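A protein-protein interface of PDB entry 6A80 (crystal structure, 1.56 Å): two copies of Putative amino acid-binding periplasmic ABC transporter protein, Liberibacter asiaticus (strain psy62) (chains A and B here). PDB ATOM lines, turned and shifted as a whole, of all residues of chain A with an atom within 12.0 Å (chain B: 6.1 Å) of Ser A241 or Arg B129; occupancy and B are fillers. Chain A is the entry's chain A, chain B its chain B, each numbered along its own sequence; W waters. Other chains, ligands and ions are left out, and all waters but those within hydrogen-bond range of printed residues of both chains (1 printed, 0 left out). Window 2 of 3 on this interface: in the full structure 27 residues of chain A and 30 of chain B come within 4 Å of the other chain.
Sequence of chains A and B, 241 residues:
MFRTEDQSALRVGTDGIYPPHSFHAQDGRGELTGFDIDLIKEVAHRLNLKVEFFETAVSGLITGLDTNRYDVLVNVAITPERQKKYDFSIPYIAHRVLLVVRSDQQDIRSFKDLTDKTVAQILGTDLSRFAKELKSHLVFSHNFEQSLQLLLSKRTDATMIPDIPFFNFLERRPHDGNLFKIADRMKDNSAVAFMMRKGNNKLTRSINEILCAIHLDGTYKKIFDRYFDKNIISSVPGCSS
Hydrophobic or aromatic side chains of chain A that line the printed part of chain B: Leu A216.
Along chain A the printed residues that touch a printed residue of chain B span positions 209 to 241.
Printed residues of chain B that touch a printed residue of chain A: Ile B78, Thr B79, Pro B80, Asp B126 and Arg B129.
Hydrophobic or aromatic side chains of chain B within 4 Å of the printed part of chain A: Ile B78 and Pro B80.
Of the printed residues of chain B, Glu A209 touches Pro B80.
Printed residues of chain B within 4 Å of Cys A212: Ile B78.
Of the printed residues of chain B, Cys A239 touches Ile B78 (3.8 Å).
Of the printed residues of chain B, Ser A241 touches Asp B126 and Arg B129.
Of the printed residues of chain A, Pro B80 touches Glu A209, Leu A216 and Ser A240.
No residue of chain A comes within 4 Å of Gly B124.
No residue of chain A comes within 4 Å of Thr B125.
Of chain A, only Ser A241 comes within 4 Å of Arg B129.
No residue of chain A comes within 4 Å of Ala B131.
No residue of chain A comes within 4 Å of Lys B132.
The nearest residue of chain A that does not touch Arg B129 is Ser A240 (6.9 Å).
The nearest printed residue of chain A that does not touch Ile B78 is Ser A241 (5.2 Å).
The side-chain sulfur (SG) of Cys A212 is disulfide-bonded to the side-chain sulfur (SG) of Cys A239 (2.1 Å).
The guanidinium group (NH1) of Arg B129 lies within hydrogen-bond range of the backbone carbonyl oxygen (O) of Asp B126, at 3.1 Å.
The side-chain carboxylate (OE2) of Glu B133 is in salt-bridge range of the guanidinium group (NE) of Arg B129, at 2.8 Å.
Among the printed residues, pairs that only touch across the chains: Ser A240 with Pro B80 (3.3 Å), Ser A240 with Thr B79 (3.3 Å), Glu A209 with Pro B80 (3.5 Å), Cys A212 with Ile B78 (3.6 Å), Leu A216 with Pro B80 (3.6 Å), Ser A241 with Asp B126 (3.7 Å) and Cys A239 with Ile B78 (3.8 Å).
Water W1 bridges O of Ile B78 (2.7 Å) and OG of Ser A240 (2.8 Å).
O of Ile B78 lies within hydrogen-bond range of N of Ser A240 (3.1 Å).
O of Ser A241 is in hydrogen-bond range of NH1 of Arg B129, at 3.3 Å.
No position is printed for both chains.
Of the 9 pairs that touch across the chains among the printed residues, none has its exchanged pair printed and touching as well.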
ATOM      1  N   ARG A  46      20.230  17.608   0.016  1.00  0.00           N
ATOM      2  CA  ARG A  46      20.300  16.348   0.722  1.00  0.00           C
ATOM      3  C   ARG A  46      18.973  15.623   0.708  1.00  0.00           C
ATOM      4  O   ARG A  46      18.925  14.414   0.964  1.00  0.00           O
ATOM      5  CB  ARG A  46      20.781  16.560   2.146  1.00  0.00           C
ATOM      6  CG  ARG A  46      22.215  16.980   2.249  1.00  0.00           C
ATOM      7  CD  ARG A  46      22.596  17.035   3.717  1.00  0.00           C
ATOM      8  NE  ARG A  46      23.923  17.617   3.846  1.00  0.00           N
ATOM      9  CZ  ARG A  46      24.778  17.298   4.803  1.00  0.00           C
ATOM     10  NH1 ARG A  46      24.474  16.355   5.682  1.00  0.00           N
ATOM     11  NH2 ARG A  46      25.964  17.909   4.862  1.00  0.00           N
ATOM     12  N   ASN A 208      13.981  18.178   9.433  1.00  0.00           N
ATOM     13  CA  ASN A 208      14.587  18.012  10.767  1.00  0.00           C
ATOM     14  C   ASN A 208      15.724  17.019  10.759  1.00  0.00           C
ATOM     15  O   ASN A 208      16.811  17.270  11.303  1.00  0.00           O
ATOM     16  CB  ASN A 208      13.564  17.690  11.848  1.00  0.00           C
ATOM     17  CG  ASN A 208      12.612  18.820  12.101  1.00  0.00           C
ATOM     18  OD1 ASN A 208      12.862  19.942  11.654  1.00  0.00           O
ATOM     19  ND2 ASN A 208      11.585  18.585  12.875  1.00  0.00           N
ATOM     20  N   GLU A 209      15.468  15.852  10.205  1.00  0.00           N
ATOM     21  CA  GLU A 209      16.468  14.820  10.166  1.00  0.00           C
ATOM     22  C   GLU A 209      17.698  15.307   9.418  1.00  0.00           C
ATOM     23  O   GLU A 209      18.878  15.108   9.863  1.00  0.00           O
ATOM     24  CB  GLU A 209      15.834  13.649   9.412  1.00  0.00           C
ATOM     25  CG  GLU A 209      16.680  12.445   9.553  1.00  0.00           C
ATOM     26  CD  GLU A 209      16.330  11.463   8.468  1.00  0.00           C
ATOM     27  OE1 GLU A 209      15.145  11.471   8.014  1.00  0.00           O
ATOM     28  OE2 GLU A 209      17.279  10.749   8.094  1.00  0.00           O
ATOM     29  N   ILE A 210      17.476  16.033   8.318  1.00  0.00           N
ATOM     30  CA  ILE A 210      18.576  16.585   7.532  1.00  0.00           C
ATOM     31  C   ILE A 210      19.334  17.718   8.255  1.00  0.00           C
ATOM     32  O   ILE A 210      20.574  17.808   8.141  1.00  0.00           O
ATOM     33  CB  ILE A 210      18.070  17.056   6.152  1.00  0.00           C
ATOM     34  CG1 ILE A 210      17.735  15.877   5.250  1.00  0.00           C
ATOM     35  CG2 ILE A 210      19.070  17.952   5.455  1.00  0.00           C
ATOM     36  CD1 ILE A 210      18.802  14.833   5.249  1.00  0.00           C
ATOM     37  N   LEU A 211      18.609  18.603   8.987  1.00  0.00           N
ATOM     38  CA  LEU A 211      19.288  19.611   9.826  1.00  0.00           C
ATOM     39  C   LEU A 211      20.211  18.885  10.858  1.00  0.00           C
ATOM     40  O   LEU A 211      21.354  19.338  11.029  1.00  0.00           O
ATOM     41  CB  LEU A 211      18.297  20.570  10.512  1.00  0.00           C
ATOM     42  CG  LEU A 211      17.676  21.618   9.560  1.00  0.00           C
ATOM     43  CD1 LEU A 211      16.489  22.203  10.309  1.00  0.00           C
ATOM     44  CD2 LEU A 211      18.769  22.628   9.188  1.00  0.00           C
ATOM     45  N   CYS A 212      19.762  17.790  11.488  1.00  0.00           N
ATOM     46  CA  CYS A 212      20.647  17.080  12.419  1.00  0.00           C
ATOM     47  C   CYS A 212      21.887  16.504  11.695  1.00  0.00           C
ATOM     48  O   CYS A 212      23.040  16.581  12.175  1.00  0.00           O
ATOM     49  CB  CYS A 212      19.886  16.036  13.236  1.00  0.00           C
ATOM     50  SG  CYS A 212      19.042  16.646  14.703  1.00  0.00           S
ATOM     51  N   ALA A 213      21.686  15.975  10.502  1.00  0.00           N
ATOM     52  CA  ALA A 213      22.808  15.496   9.750  1.00  0.00           C
ATOM     53  C   ALA A 213      23.835  16.578   9.396  1.00  0.00           C
ATOM     54  O   ALA A 213      25.047  16.352   9.329  1.00  0.00           O
ATOM     55  CB  ALA A 213      22.317  14.762   8.484  1.00  0.00           C
ATOM     56  N   ILE A 214      23.310  17.790   9.143  1.00  0.00           N
ATOM     57  CA  ILE A 214      24.139  18.907   8.819  1.00  0.00           C
ATOM     58  C   ILE A 214      24.913  19.387  10.024  1.00  0.00           C
ATOM     59  O   ILE A 214      26.072  19.787   9.862  1.00  0.00           O
ATOM     60  CB  ILE A 214      23.192  20.006   8.238  1.00  0.00           C
ATOM     61  CG1 ILE A 214      22.837  19.629   6.805  1.00  0.00           C
ATOM     62  CG2 ILE A 214      23.819  21.391   8.225  1.00  0.00           C
ATOM     63  CD1 ILE A 214      21.690  20.504   6.224  1.00  0.00           C
ATOM     64  N   HIS A 215      24.328  19.314  11.202  1.00  0.00           N
ATOM     65  CA  HIS A 215      25.077  19.579  12.480  1.00  0.00           C
ATOM     66  C   HIS A 215      26.199  18.545  12.634  1.00  0.00           C
ATOM     67  O   HIS A 215      27.375  18.916  12.869  1.00  0.00           O
ATOM     68  CB  HIS A 215      24.115  19.475  13.663  1.00  0.00           C
ATOM     69  CG  HIS A 215      23.339  20.733  13.937  1.00  0.00           C
ATOM     70  ND1 HIS A 215      23.909  21.834  14.551  1.00  0.00           N
ATOM     71  CD2 HIS A 215      22.037  21.044  13.710  1.00  0.00           C
ATOM     72  CE1 HIS A 215      22.989  22.774  14.695  1.00  0.00           C
ATOM     73  NE2 HIS A 215      21.843  22.334  14.182  1.00  0.00           N
ATOM     74  N   LEU A 216      25.836  17.281  12.419  1.00  0.00           N
ATOM     75  CA  LEU A 216      26.778  16.178  12.833  1.00  0.00           C
ATOM     76  C   LEU A 216      28.000  16.145  11.970  1.00  0.00           C
ATOM     77  O   LEU A 216      29.101  15.774  12.477  1.00  0.00           O
ATOM     78  CB  LEU A 216      26.057  14.816  12.876  1.00  0.00           C
ATOM     79  CG  LEU A 216      25.051  14.666  14.002  1.00  0.00           C
ATOM     80  CD1 LEU A 216      24.086  13.524  13.659  1.00  0.00           C
ATOM     81  CD2 LEU A 216      25.795  14.318  15.307  1.00  0.00           C
ATOM     82  N   ASP A 217      27.890  16.518  10.711  1.00  0.00           N
ATOM     83  CA  ASP A 217      29.026  16.432   9.873  1.00  0.00           C
ATOM     84  C   ASP A 217      29.871  17.659   9.756  1.00  0.00           C
ATOM     85  O   ASP A 217      30.803  17.669   8.932  1.00  0.00           O
ATOM     86  CB  ASP A 217      28.711  15.813   8.516  1.00  0.00           C
ATOM     87  CG  ASP A 217      28.024  16.776   7.562  1.00  0.00           C
ATOM     88  OD1 ASP A 217      27.826  17.971   7.902  1.00  0.00           O
ATOM     89  OD2 ASP A 217      27.681  16.326   6.458  1.00  0.00           O
ATOM     90  N   GLY A 218      29.598  18.657  10.629  1.00  0.00           N
ATOM     91  CA  GLY A 218      30.346  19.906  10.628  1.00  0.00           C
ATOM     92  C   GLY A 218      29.836  20.943   9.636  1.00  0.00           C
ATOM     93  O   GLY A 218      30.413  22.012   9.544  1.00  0.00           O
ATOM     94  N   PRO A 237      21.713  24.092  19.907  1.00  0.00           N
ATOM     95  CA  PRO A 237      22.473  22.844  20.187  1.00  0.00           C
ATOM     96  C   PRO A 237      22.653  22.009  18.995  1.00  0.00           C
ATOM     97  O   PRO A 237      21.854  22.135  18.050  1.00  0.00           O
ATOM     98  CB  PRO A 237      21.614  22.153  21.247  1.00  0.00           C
ATOM     99  CG  PRO A 237      20.301  22.798  21.193  1.00  0.00           C
ATOM    100  CD  PRO A 237      20.498  24.204  20.699  1.00  0.00           C
ATOM    101  N   GLY A 238      23.687  21.160  18.982  1.00  0.00           N
ATOM    102  CA  GLY A 238      23.811  20.206  17.915  1.00  0.00           C
ATOM    103  C   GLY A 238      22.937  18.992  18.190  1.00  0.00           C
ATOM    104  O   GLY A 238      21.992  19.045  19.016  1.00  0.00           O
ATOM    105  N   CYS A 239      23.169  17.930  17.430  1.00  0.00           N
ATOM    106  CA  CYS A 239      22.433  16.679  17.580  1.00  0.00           C
ATOM    107  C   CYS A 239      23.434  15.551  17.831  1.00  0.00           C
ATOM    108  O   CYS A 239      24.651  15.763  17.844  1.00  0.00           O
ATOM    109  CB  CYS A 239      21.627  16.326  16.347  1.00  0.00           C
ATOM    110  SG  CYS A 239      20.529  17.630  15.745  1.00  0.00           S
ATOM    111  N   SER A 240      22.886  14.362  18.056  1.00  0.00           N
ATOM    112  CA  SER A 240      23.663  13.209  18.535  1.00  0.00           C
ATOM    113  C   SER A 240      23.527  12.118  17.469  1.00  0.00           C
ATOM    114  O   SER A 240      22.646  12.126  16.682  1.00  0.00           O
ATOM    115  CB  SER A 240      23.073  12.659  19.835  1.00  0.00           C
ATOM    116  OG  SER A 240      23.149  13.672  20.843  1.00  0.00           O
ATOM    117  N   SER A 241      24.385  11.138  17.502  1.00  0.00           N
ATOM    118  CA  SER A 241      24.054   9.978  16.643  1.00  0.00           C
ATOM    119  C   SER A 241      24.084   8.666  17.427  1.00  0.00           C
ATOM    120  O   SER A 241      24.371   8.689  18.640  1.00  0.00           O
ATOM    121  CB  SER A 241      25.018   9.966  15.503  1.00  0.00           C
ATOM    122  OG  SER A 241      26.348   9.864  15.968  1.00  0.00           O
ATOM    123  N   ILE B  78      18.044  13.953  20.644  1.00  0.00           N
ATOM    124  CA  ILE B  78      17.653  13.857  19.230  1.00  0.00           C
ATOM    125  C   ILE B  78      18.770  13.287  18.406  1.00  0.00           C
ATOM    126  O   ILE B  78      19.932  13.700  18.515  1.00  0.00           O
ATOM    127  CB  ILE B  78      17.282  15.259  18.739  1.00  0.00           C
ATOM    128  CG1 ILE B  78      16.096  15.773  19.572  1.00  0.00           C
ATOM    129  CG2 ILE B  78      16.951  15.255  17.223  1.00  0.00           C
ATOM    130  CD1 ILE B  78      15.568  17.186  19.160  1.00  0.00           C
ATOM    131  N   THR B  79      18.436  12.299  17.575  1.00  0.00           N
ATOM    132  CA  THR B  79      19.375  11.706  16.619  1.00  0.00           C
ATOM    133  C   THR B  79      18.631  11.594  15.264  1.00  0.00           C
ATOM    134  O   THR B  79      17.404  11.542  15.286  1.00  0.00           O
ATOM    135  CB  THR B  79      19.852  10.312  17.007  1.00  0.00           C
ATOM    136  OG1 THR B  79      18.740   9.366  16.910  1.00  0.00           O
ATOM    137  CG2 THR B  79      20.337  10.310  18.528  1.00  0.00           C
ATOM    138  N   PRO B  80      19.387  11.596  14.142  1.00  0.00           N
ATOM    139  CA  PRO B  80      18.698  11.513  12.840  1.00  0.00           C
ATOM    140  C   PRO B  80      17.907  10.177  12.705  1.00  0.00           C
ATOM    141  O   PRO B  80      16.790  10.193  12.185  1.00  0.00           O
ATOM    142  CB  PRO B  80      19.826  11.497  11.825  1.00  0.00           C
ATOM    143  CG  PRO B  80      21.072  11.840  12.492  1.00  0.00           C
ATOM    144  CD  PRO B  80      20.820  11.847  13.992  1.00  0.00           C
ATOM    145  N   GLU B  81      18.474   9.098  13.245  1.00  0.00           N
ATOM    146  CA  GLU B  81      17.849   7.765  13.252  1.00  0.00           C
ATOM    147  C   GLU B  81      16.563   7.720  14.121  1.00  0.00           C
ATOM    148  O   GLU B  81      15.600   7.010  13.792  1.00  0.00           O
ATOM    149  CB  GLU B  81      18.924   6.742  13.673  1.00  0.00           C
ATOM    150  CG  GLU B  81      20.214   6.810  12.812  1.00  0.00           C
ATOM    151  CD  GLU B  81      21.287   7.869  13.232  1.00  0.00           C
ATOM    152  OE1 GLU B  81      21.157   8.556  14.271  1.00  0.00           O
ATOM    153  OE2 GLU B  81      22.306   8.023  12.505  1.00  0.00           O
ATOM    154  N   GLN B 121      28.793   1.435  30.555  1.00  0.00           N
ATOM    155  CA  GLN B 121      27.712   2.151  29.839  1.00  0.00           C
ATOM    156  C   GLN B 121      26.414   1.450  30.112  1.00  0.00           C
ATOM    157  O   GLN B 121      26.382   0.265  30.530  1.00  0.00           O
ATOM    158  CB  GLN B 121      27.921   2.239  28.327  1.00  0.00           C
ATOM    159  CG  GLN B 121      29.269   2.812  27.902  1.00  0.00           C
ATOM    160  CD  GLN B 121      29.455   4.285  28.152  1.00  0.00           C
ATOM    161  OE1 GLN B 121      30.601   4.718  28.178  1.00  0.00           O
ATOM    162  NE2 GLN B 121      28.359   5.038  28.383  1.00  0.00           N
ATOM    163  N   GLY B 124      21.653  -0.808  26.274  1.00  0.00           N
ATOM    164  CA  GLY B 124      20.715  -0.346  25.272  1.00  0.00           C
ATOM    165  C   GLY B 124      20.737   1.154  24.944  1.00  0.00           C
ATOM    166  O   GLY B 124      19.808   1.667  24.320  1.00  0.00           O
ATOM    167  N   THR B 125      21.786   1.865  25.368  1.00  0.00           N
ATOM    168  CA  THR B 125      21.854   3.297  25.049  1.00  0.00           C
ATOM    169  C   THR B 125      22.710   3.536  23.817  1.00  0.00           C
ATOM    170  O   THR B 125      23.564   2.695  23.478  1.00  0.00           O
ATOM    171  CB  THR B 125      22.399   4.101  26.216  1.00  0.00           C
ATOM    172  OG1 THR B 125      23.717   3.637  26.562  1.00  0.00           O
ATOM    173  CG2 THR B 125      21.445   3.964  27.460  1.00  0.00           C
ATOM    174  N   ASP B 126      22.521   4.685  23.144  1.00  0.00           N
ATOM    175  CA  ASP B 126      23.434   5.078  22.061  1.00  0.00           C
ATOM    176  C   ASP B 126      24.890   5.138  22.508  1.00  0.00           C
ATOM    177  O   ASP B 126      25.789   4.814  21.689  1.00  0.00           O
ATOM    178  CB  ASP B 126      23.001   6.420  21.449  1.00  0.00           C
ATOM    179  CG  ASP B 126      21.798   6.263  20.508  1.00  0.00           C
ATOM    180  OD1 ASP B 126      21.390   5.116  20.219  1.00  0.00           O
ATOM    181  OD2 ASP B 126      21.232   7.300  20.093  1.00  0.00           O
ATOM    182  N   LEU B 127      25.167   5.564  23.739  1.00  0.00           N
ATOM    183  CA  LEU B 127      26.582   5.613  24.130  1.00  0.00           C
ATOM    184  C   LEU B 127      27.156   4.185  24.370  1.00  0.00           C
ATOM    185  O   LEU B 127      28.352   3.952  24.179  1.00  0.00           O
ATOM    186  CB  LEU B 127      26.749   6.522  25.367  1.00  0.00           C
ATOM    187  CG  LEU B 127      26.651   8.025  24.982  1.00  0.00           C
ATOM    188  CD1 LEU B 127      26.792   8.794  26.298  1.00  0.00           C
ATOM    189  CD2 LEU B 127      27.793   8.374  24.047  1.00  0.00           C
ATOM    190  N   SER B 128      26.304   3.240  24.798  1.00  0.00           N
ATOM    191  CA  SER B 128      26.765   1.852  24.893  1.00  0.00           C
ATOM    192  C   SER B 128      27.110   1.348  23.476  1.00  0.00           C
ATOM    193  O   SER B 128      28.136   0.713  23.274  1.00  0.00           O
ATOM    194  CB  SER B 128      25.710   0.976  25.555  1.00  0.00           C
ATOM    195  OG  SER B 128      26.126  -0.385  25.548  1.00  0.00           O
ATOM    196  N   ARG B 129      26.243   1.653  22.516  1.00  0.00           N
ATOM    197  CA  ARG B 129      26.468   1.256  21.091  1.00  0.00           C
ATOM    198  C   ARG B 129      27.806   1.850  20.590  1.00  0.00           C
ATOM    199  O   ARG B 129      28.581   1.186  19.903  1.00  0.00           O
ATOM    200  CB  ARG B 129      25.266   1.688  20.230  1.00  0.00           C
ATOM    201  CG  ARG B 129      25.409   1.520  18.716  1.00  0.00           C
ATOM    202  CD  ARG B 129      24.847   2.714  17.889  1.00  0.00           C
ATOM    203  NE  ARG B 129      25.888   3.705  17.496  1.00  0.00           N
ATOM    204  CZ  ARG B 129      25.991   4.976  17.923  1.00  0.00           C
ATOM    205  NH1 ARG B 129      25.108   5.501  18.761  1.00  0.00           N
ATOM    206  NH2 ARG B 129      27.001   5.734  17.499  1.00  0.00           N
ATOM    207  N   PHE B 130      28.093   3.097  20.961  1.00  0.00           N
ATOM    208  CA  PHE B 130      29.325   3.748  20.499  1.00  0.00           C
ATOM    209  C   PHE B 130      30.514   3.052  21.120  1.00  0.00           C
ATOM    210  O   PHE B 130      31.511   2.799  20.422  1.00  0.00           O
ATOM    211  CB  PHE B 130      29.256   5.250  20.887  1.00  0.00           C
ATOM    212  CG  PHE B 130      30.462   6.071  20.479  1.00  0.00           C
ATOM    213  CD1 PHE B 130      31.078   5.962  19.208  1.00  0.00           C
ATOM    214  CD2 PHE B 130      30.958   6.964  21.392  1.00  0.00           C
ATOM    215  CE1 PHE B 130      32.197   6.771  18.883  1.00  0.00           C
ATOM    216  CE2 PHE B 130      32.047   7.779  21.068  1.00  0.00           C
ATOM    217  CZ  PHE B 130      32.664   7.680  19.845  1.00  0.00           C
ATOM    218  N   ALA B 131      30.421   2.720  22.429  1.00  0.00           N
ATOM    219  CA  ALA B 131      31.523   1.990  23.064  1.00  0.00           C
ATOM    220  C   ALA B 131      31.804   0.610  22.341  1.00  0.00           C
ATOM    221  O   ALA B 131      32.948   0.165  22.190  1.00  0.00           O
ATOM    222  CB  ALA B 131      31.231   1.777  24.583  1.00  0.00           C
ATOM    223  N   LYS B 132      30.734  -0.052  21.964  1.00  0.00           N
ATOM    224  CA  LYS B 132      30.821  -1.320  21.256  1.00  0.00           C
ATOM    225  C   LYS B 132      31.438  -1.078  19.883  1.00  0.00           C
ATOM    226  O   LYS B 132      32.296  -1.834  19.455  1.00  0.00           O
ATOM    227  CB  LYS B 132      29.464  -1.936  21.072  1.00  0.00           C
ATOM    228  CG  LYS B 132      28.779  -2.467  22.306  1.00  0.00           C
ATOM    229  CD  LYS B 132      27.428  -2.955  21.821  1.00  0.00           C
ATOM    230  CE  LYS B 132      26.593  -3.571  22.916  1.00  0.00           C
ATOM    231  NZ  LYS B 132      25.297  -3.979  22.287  1.00  0.00           N
ATOM    232  N   GLU B 133      31.078   0.016  19.222  1.00  0.00           N
ATOM    233  CA  GLU B 133      31.724   0.329  17.943  1.00  0.00           C
ATOM    234  C   GLU B 133      33.203   0.610  18.076  1.00  0.00           C
ATOM    235  O   GLU B 133      33.986   0.255  17.173  1.00  0.00           O
ATOM    236  CB  GLU B 133      31.029   1.517  17.280  1.00  0.00           C
ATOM    237  CG  GLU B 133      29.672   1.153  16.706  1.00  0.00           C
ATOM    238  CD  GLU B 133      28.759   2.374  16.426  1.00  0.00           C
ATOM    239  OE1 GLU B 133      29.144   3.561  16.636  1.00  0.00           O
ATOM    240  OE2 GLU B 133      27.605   2.119  16.033  1.00  0.00           O
ATOM    241  N   LEU B 134      33.625   1.230  19.203  1.00  0.00           N
ATOM    242  CA  LEU B 134      35.019   1.481  19.467  1.00  0.00           C
ATOM    243  C   LEU B 134      35.787   0.201  19.881  1.00  0.00           C
ATOM    244  O   LEU B 134      36.991   0.277  20.085  1.00  0.00           O
ATOM    245  CB  LEU B 134      35.134   2.516  20.598  1.00  0.00           C
ATOM    246  CG  LEU B 134      34.773   3.958  20.252  1.00  0.00           C
ATOM    247  CD1 LEU B 134      34.607   4.732  21.561  1.00  0.00           C
ATOM    248  CD2 LEU B 134      35.890   4.513  19.337  1.00  0.00           C
HETATM  249  O   HOH W   1      21.015  15.378  20.391  1.00  0.00           O
